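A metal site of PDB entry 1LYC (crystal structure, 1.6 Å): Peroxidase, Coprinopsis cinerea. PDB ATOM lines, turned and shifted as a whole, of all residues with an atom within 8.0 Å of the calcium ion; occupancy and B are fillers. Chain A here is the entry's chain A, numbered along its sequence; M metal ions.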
ATOM      1  N   PRO A 129      29.519 -15.862 -27.294  1.00  0.00           N
ATOM      2  CA  PRO A 129      30.610 -16.336 -26.428  1.00  0.00           C
ATOM      3  C   PRO A 129      30.150 -16.989 -25.125  1.00  0.00           C
ATOM      4  O   PRO A 129      29.302 -16.447 -24.426  1.00  0.00           O
ATOM      5  CB  PRO A 129      31.429 -15.078 -26.183  1.00  0.00           C
ATOM      6  CG  PRO A 129      31.249 -14.306 -27.467  1.00  0.00           C
ATOM      7  CD  PRO A 129      29.785 -14.483 -27.756  1.00  0.00           C
ATOM      8  N   ALA A 181      18.327 -19.732 -18.407  1.00  0.00           N
ATOM      9  CA  ALA A 181      19.709 -19.284 -18.564  1.00  0.00           C
ATOM     10  C   ALA A 181      19.738 -18.515 -19.896  1.00  0.00           C
ATOM     11  O   ALA A 181      20.689 -17.793 -20.188  1.00  0.00           O
ATOM     12  CB  ALA A 181      20.661 -20.474 -18.627  1.00  0.00           C
ATOM     13  N   ALA A 182      18.665 -18.669 -20.673  1.00  0.00           N
ATOM     14  CA  ALA A 182      18.505 -18.002 -21.960  1.00  0.00           C
ATOM     15  C   ALA A 182      18.394 -16.478 -21.797  1.00  0.00           C
ATOM     16  O   ALA A 182      18.714 -15.729 -22.722  1.00  0.00           O
ATOM     17  CB  ALA A 182      17.262 -18.553 -22.677  1.00  0.00           C
ATOM     18  N   HIS A 183      17.927 -16.034 -20.625  1.00  0.00           N
ATOM     19  CA  HIS A 183      17.798 -14.603 -20.361  1.00  0.00           C
ATOM     20  C   HIS A 183      19.166 -13.942 -20.165  1.00  0.00           C
ATOM     21  O   HIS A 183      19.255 -12.734 -19.905  1.00  0.00           O
ATOM     22  CB  HIS A 183      16.930 -14.359 -19.123  1.00  0.00           C
ATOM     23  CG  HIS A 183      15.452 -14.402 -19.403  1.00  0.00           C
ATOM     24  ND1 HIS A 183      14.478 -14.018 -18.512  1.00  0.00           N
ATOM     25  CD2 HIS A 183      14.795 -14.791 -20.519  1.00  0.00           C
ATOM     26  CE1 HIS A 183      13.288 -14.191 -19.084  1.00  0.00           C
ATOM     27  NE2 HIS A 183      13.428 -14.652 -20.311  1.00  0.00           N
ATOM     28  N   SER A 184      20.230 -14.736 -20.299  1.00  0.00           N
ATOM     29  CA  SER A 184      21.595 -14.248 -20.212  1.00  0.00           C
ATOM     30  C   SER A 184      21.934 -13.533 -21.544  1.00  0.00           C
ATOM     31  O   SER A 184      22.886 -12.764 -21.624  1.00  0.00           O
ATOM     32  CB  SER A 184      22.564 -15.406 -19.996  1.00  0.00           C
ATOM     33  OG  SER A 184      23.872 -14.937 -19.734  1.00  0.00           O
ATOM     34  N   LEU A 185      21.139 -13.813 -22.566  1.00  0.00           N
ATOM     35  CA  LEU A 185      21.307 -13.209 -23.890  1.00  0.00           C
ATOM     36  C   LEU A 185      19.927 -12.643 -24.256  1.00  0.00           C
ATOM     37  O   LEU A 185      19.299 -13.086 -25.215  1.00  0.00           O
ATOM     38  CB  LEU A 185      21.706 -14.286 -24.906  1.00  0.00           C
ATOM     39  CG  LEU A 185      22.949 -15.139 -24.634  1.00  0.00           C
ATOM     40  CD1 LEU A 185      23.097 -16.199 -25.723  1.00  0.00           C
ATOM     41  CD2 LEU A 185      24.182 -14.258 -24.572  1.00  0.00           C
ATOM     42  N   ALA A 186      19.478 -11.629 -23.506  1.00  0.00           N
ATOM     43  CA  ALA A 186      18.145 -11.087 -23.727  1.00  0.00           C
ATOM     44  C   ALA A 186      17.931  -9.622 -23.369  1.00  0.00           C
ATOM     45  O   ALA A 186      18.737  -9.000 -22.695  1.00  0.00           O
ATOM     46  CB  ALA A 186      17.149 -11.937 -22.960  1.00  0.00           C
ATOM     47  N   LEU A 200      18.591  -7.717 -19.950  1.00  0.00           N
ATOM     48  CA  LEU A 200      18.120  -8.412 -18.770  1.00  0.00           C
ATOM     49  C   LEU A 200      19.306  -8.681 -17.839  1.00  0.00           C
ATOM     50  O   LEU A 200      19.132  -8.988 -16.666  1.00  0.00           O
ATOM     51  CB  LEU A 200      17.408  -9.717 -19.153  1.00  0.00           C
ATOM     52  CG  LEU A 200      15.903  -9.627 -19.421  1.00  0.00           C
ATOM     53  CD1 LEU A 200      15.556  -8.357 -20.183  1.00  0.00           C
ATOM     54  CD2 LEU A 200      15.464 -10.856 -20.182  1.00  0.00           C
ATOM     55  N   ASP A 201      20.519  -8.568 -18.391  1.00  0.00           N
ATOM     56  CA  ASP A 201      21.764  -8.708 -17.628  1.00  0.00           C
ATOM     57  C   ASP A 201      22.861  -7.870 -18.322  1.00  0.00           C
ATOM     58  O   ASP A 201      22.710  -7.485 -19.492  1.00  0.00           O
ATOM     59  CB  ASP A 201      22.163 -10.195 -17.445  1.00  0.00           C
ATOM     60  CG  ASP A 201      23.020 -10.759 -18.566  1.00  0.00           C
ATOM     61  OD1 ASP A 201      23.292 -10.073 -19.566  1.00  0.00           O
ATOM     62  OD2 ASP A 201      23.444 -11.926 -18.442  1.00  0.00           O
ATOM     63  N   SER A 202      23.934  -7.574 -17.599  1.00  0.00           N
ATOM     64  CA  SER A 202      25.029  -6.743 -18.130  1.00  0.00           C
ATOM     65  C   SER A 202      25.755  -7.240 -19.365  1.00  0.00           C
ATOM     66  O   SER A 202      26.542  -6.498 -19.957  1.00  0.00           O
ATOM     67  CB  SER A 202      26.048  -6.466 -17.024  1.00  0.00           C
ATOM     68  OG  SER A 202      26.563  -7.687 -16.506  1.00  0.00           O
ATOM     69  N   THR A 203      25.517  -8.492 -19.761  1.00  0.00           N
ATOM     70  CA  THR A 203      26.176  -9.065 -20.935  1.00  0.00           C
ATOM     71  C   THR A 203      25.214  -9.839 -21.862  1.00  0.00           C
ATOM     72  O   THR A 203      25.299 -11.072 -21.986  1.00  0.00           O
ATOM     73  CB  THR A 203      27.337 -10.004 -20.495  1.00  0.00           C
ATOM     74  OG1 THR A 203      26.871 -10.916 -19.498  1.00  0.00           O
ATOM     75  CG2 THR A 203      28.469  -9.206 -19.931  1.00  0.00           C
ATOM     76  N   PRO A 204      24.289  -9.132 -22.535  1.00  0.00           N
ATOM     77  CA  PRO A 204      23.329  -9.763 -23.443  1.00  0.00           C
ATOM     78  C   PRO A 204      23.940 -10.416 -24.697  1.00  0.00           C
ATOM     79  O   PRO A 204      23.217 -10.953 -25.539  1.00  0.00           O
ATOM     80  CB  PRO A 204      22.361  -8.621 -23.782  1.00  0.00           C
ATOM     81  CG  PRO A 204      23.234  -7.415 -23.710  1.00  0.00           C
ATOM     82  CD  PRO A 204      24.064  -7.668 -22.467  1.00  0.00           C
ATOM     83  N   GLN A 205      25.271 -10.362 -24.812  1.00  0.00           N
ATOM     84  CA  GLN A 205      25.980 -10.961 -25.941  1.00  0.00           C
ATOM     85  C   GLN A 205      26.992 -12.014 -25.485  1.00  0.00           C
ATOM     86  O   GLN A 205      27.860 -12.433 -26.255  1.00  0.00           O
ATOM     87  CB  GLN A 205      26.707  -9.912 -26.769  1.00  0.00           C
ATOM     88  CG  GLN A 205      25.806  -9.098 -27.678  1.00  0.00           C
ATOM     89  CD  GLN A 205      26.594  -8.238 -28.636  1.00  0.00           C
ATOM     90  OE1 GLN A 205      27.378  -7.383 -28.213  1.00  0.00           O
ATOM     91  NE2 GLN A 205      26.396  -8.449 -29.941  1.00  0.00           N
ATOM     92  N   VAL A 206      26.864 -12.424 -24.218  1.00  0.00           N
ATOM     93  CA  VAL A 206      27.731 -13.443 -23.638  1.00  0.00           C
ATOM     94  C   VAL A 206      26.895 -14.374 -22.766  1.00  0.00           C
ATOM     95  O   VAL A 206      26.270 -13.928 -21.791  1.00  0.00           O
ATOM     96  CB  VAL A 206      28.845 -12.826 -22.768  1.00  0.00           C
ATOM     97  CG1 VAL A 206      29.699 -13.942 -22.168  1.00  0.00           C
ATOM     98  CG2 VAL A 206      29.695 -11.895 -23.583  1.00  0.00           C
ATOM     99  N   PHE A 207      26.886 -15.654 -23.104  1.00  0.00           N
ATOM    100  CA  PHE A 207      26.133 -16.643 -22.345  1.00  0.00           C
ATOM    101  C   PHE A 207      26.878 -16.933 -21.048  1.00  0.00           C
ATOM    102  O   PHE A 207      27.812 -17.741 -21.022  1.00  0.00           O
ATOM    103  CB  PHE A 207      25.961 -17.921 -23.164  1.00  0.00           C
ATOM    104  CG  PHE A 207      25.061 -18.938 -22.517  1.00  0.00           C
ATOM    105  CD1 PHE A 207      23.685 -18.739 -22.480  1.00  0.00           C
ATOM    106  CD2 PHE A 207      25.602 -20.069 -21.916  1.00  0.00           C
ATOM    107  CE1 PHE A 207      22.850 -19.654 -21.835  1.00  0.00           C
ATOM    108  CE2 PHE A 207      24.775 -20.996 -21.272  1.00  0.00           C
ATOM    109  CZ  PHE A 207      23.405 -20.784 -21.235  1.00  0.00           C
ATOM    110  N   ASP A 208      26.474 -16.267 -19.969  1.00  0.00           N
ATOM    111  CA  ASP A 208      27.113 -16.423 -18.663  1.00  0.00           C
ATOM    112  C   ASP A 208      26.125 -16.357 -17.498  1.00  0.00           C
ATOM    113  O   ASP A 208      24.926 -16.128 -17.701  1.00  0.00           O
ATOM    114  CB  ASP A 208      28.193 -15.354 -18.472  1.00  0.00           C
ATOM    115  CG  ASP A 208      27.649 -13.960 -18.719  1.00  0.00           C
ATOM    116  OD1 ASP A 208      26.421 -13.779 -18.590  1.00  0.00           O
ATOM    117  OD2 ASP A 208      28.446 -13.056 -19.029  1.00  0.00           O
ATOM    118  N   THR A 209      26.633 -16.526 -16.281  1.00  0.00           N
ATOM    119  CA  THR A 209      25.825 -16.519 -15.077  1.00  0.00           C
ATOM    120  C   THR A 209      25.369 -15.153 -14.580  1.00  0.00           C
ATOM    121  O   THR A 209      24.708 -15.078 -13.546  1.00  0.00           O
ATOM    122  CB  THR A 209      26.554 -17.245 -13.892  1.00  0.00           C
ATOM    123  OG1 THR A 209      27.745 -16.517 -13.531  1.00  0.00           O
ATOM    124  CG2 THR A 209      26.952 -18.669 -14.299  1.00  0.00           C
ATOM    125  N   GLN A 210      25.717 -14.085 -15.297  1.00  0.00           N
ATOM    126  CA  GLN A 210      25.344 -12.745 -14.840  1.00  0.00           C
ATOM    127  C   GLN A 210      23.854 -12.583 -14.570  1.00  0.00           C
ATOM    128  O   GLN A 210      23.464 -11.963 -13.571  1.00  0.00           O
ATOM    129  CB  GLN A 210      25.817 -11.678 -15.817  1.00  0.00           C
ATOM    130  CG  GLN A 210      27.329 -11.486 -15.841  1.00  0.00           C
ATOM    131  CD  GLN A 210      27.948 -11.339 -14.439  1.00  0.00           C
ATOM    132  OE1 GLN A 210      28.809 -12.133 -14.048  1.00  0.00           O
ATOM    133  NE2 GLN A 210      27.521 -10.320 -13.686  1.00  0.00           N
ATOM    134  N   PHE A 211      23.026 -13.123 -15.452  1.00  0.00           N
ATOM    135  CA  PHE A 211      21.577 -13.044 -15.309  1.00  0.00           C
ATOM    136  C   PHE A 211      21.124 -13.495 -13.907  1.00  0.00           C
ATOM    137  O   PHE A 211      20.349 -12.799 -13.242  1.00  0.00           O
ATOM    138  CB  PHE A 211      20.917 -13.916 -16.383  1.00  0.00           C
ATOM    139  CG  PHE A 211      19.458 -14.182 -16.125  1.00  0.00           C
ATOM    140  CD1 PHE A 211      18.528 -13.138 -16.189  1.00  0.00           C
ATOM    141  CD2 PHE A 211      19.016 -15.464 -15.776  1.00  0.00           C
ATOM    142  CE1 PHE A 211      17.169 -13.360 -15.900  1.00  0.00           C
ATOM    143  CE2 PHE A 211      17.659 -15.694 -15.481  1.00  0.00           C
ATOM    144  CZ  PHE A 211      16.735 -14.638 -15.546  1.00  0.00           C
ATOM    145  N   TYR A 212      21.578 -14.677 -13.467  1.00  0.00           N
ATOM    146  CA  TYR A 212      21.206 -15.224 -12.162  1.00  0.00           C
ATOM    147  C   TYR A 212      21.734 -14.381 -11.010  1.00  0.00           C
ATOM    148  O   TYR A 212      21.048 -14.183 -10.001  1.00  0.00           O
ATOM    149  CB  TYR A 212      21.725 -16.646 -12.013  1.00  0.00           C
ATOM    150  CG  TYR A 212      21.091 -17.626 -12.980  1.00  0.00           C
ATOM    151  CD1 TYR A 212      19.806 -18.123 -12.750  1.00  0.00           C
ATOM    152  CD2 TYR A 212      21.778 -18.071 -14.102  1.00  0.00           C
ATOM    153  CE1 TYR A 212      19.222 -19.040 -13.627  1.00  0.00           C
ATOM    154  CE2 TYR A 212      21.214 -18.991 -14.987  1.00  0.00           C
ATOM    155  CZ  TYR A 212      19.931 -19.473 -14.734  1.00  0.00           C
ATOM    156  OH  TYR A 212      19.387 -20.411 -15.575  1.00  0.00           O
ATOM    157  N   GLU A 214      22.711 -10.975 -11.103  1.00  0.00           N
ATOM    158  CA  GLU A 214      22.050  -9.680 -11.121  1.00  0.00           C
ATOM    159  C   GLU A 214      20.576  -9.652 -10.785  1.00  0.00           C
ATOM    160  O   GLU A 214      20.079  -8.646 -10.269  1.00  0.00           O
ATOM    161  CB  GLU A 214      22.332  -8.992 -12.465  1.00  0.00           C
ATOM    162  CG  GLU A 214      23.844  -8.856 -12.697  1.00  0.00           C
ATOM    163  CD  GLU A 214      24.210  -8.377 -14.092  1.00  0.00           C
ATOM    164  OE1 GLU A 214      25.417  -8.443 -14.416  1.00  0.00           O
ATOM    165  OE2 GLU A 214      23.320  -7.941 -14.851  1.00  0.00           O
ATOM    166  N   ASN A 265      30.044 -21.050 -15.063  1.00  0.00           N
ATOM    167  CA  ASN A 265      29.563 -20.910 -16.430  1.00  0.00           C
ATOM    168  C   ASN A 265      29.390 -22.298 -17.063  1.00  0.00           C
ATOM    169  O   ASN A 265      28.427 -22.531 -17.800  1.00  0.00           O
ATOM    170  CB  ASN A 265      30.527 -20.060 -17.287  1.00  0.00           C
ATOM    171  CG  ASN A 265      30.440 -18.564 -16.983  1.00  0.00           C
ATOM    172  OD1 ASN A 265      29.347 -18.001 -16.911  1.00  0.00           O
ATOM    173  ND2 ASN A 265      31.584 -17.924 -16.831  1.00  0.00           N
ATOM    174  N   MET A 268      26.221 -24.121 -15.540  1.00  0.00           N
ATOM    175  CA  MET A 268      25.036 -23.464 -16.086  1.00  0.00           C
ATOM    176  C   MET A 268      24.827 -23.962 -17.513  1.00  0.00           C
ATOM    177  O   MET A 268      23.717 -24.294 -17.900  1.00  0.00           O
ATOM    178  CB  MET A 268      25.199 -21.944 -16.085  1.00  0.00           C
ATOM    179  CG  MET A 268      24.019 -21.235 -16.739  1.00  0.00           C
ATOM    180  SD  MET A 268      24.230 -19.470 -17.061  1.00  0.00           S
ATOM    181  CE  MET A 268      25.527 -19.496 -18.302  1.00  0.00           C
ATOM    182  N   ASN A 302      34.413 -18.201 -23.163  1.00  0.00           N
ATOM    183  CA  ASN A 302      34.182 -17.084 -22.271  1.00  0.00           C
ATOM    184  C   ASN A 302      35.130 -17.319 -21.100  1.00  0.00           C
ATOM    185  O   ASN A 302      34.830 -18.125 -20.215  1.00  0.00           O
ATOM    186  CB  ASN A 302      32.745 -17.075 -21.743  1.00  0.00           C
ATOM    187  CG  ASN A 302      32.519 -16.015 -20.656  1.00  0.00           C
ATOM    188  OD1 ASN A 302      31.503 -16.038 -19.959  1.00  0.00           O
ATOM    189  ND2 ASN A 302      33.466 -15.085 -20.510  1.00  0.00           N
HETATM  190 CA    CA M   1      24.711 -12.540 -20.291  1.00  0.00          CA
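The side-chain carboxylate (OD2) of Asp 201 sits close to the backbone NH (N) of Phe 211 (3.2 Å). The side-chain carboxylate of Asp 208 lies close to the backbone NH of Gln 210, 3.4 Å away.
Five residues have an atom within 4 Å of the calcium ion: Ser 184, Asp 201, Thr 203, Val 206 and Asp 208.
The calcium ion is bound by O of Ser 184 (2.3 Å), O of Thr 203 (2.3 Å), OD2 of Asp 201 (2.3 Å), O of Val 206 (2.6 Å), OG of Ser 184 (2.6 Å), OD1 of Asp 208 (2.7 Å) and OG1 of Thr 203 (2.8 Å). Slightly farther from the calcium ion lies the side-chain carboxylate (OD1) of Asp 201 (2.9 Å).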
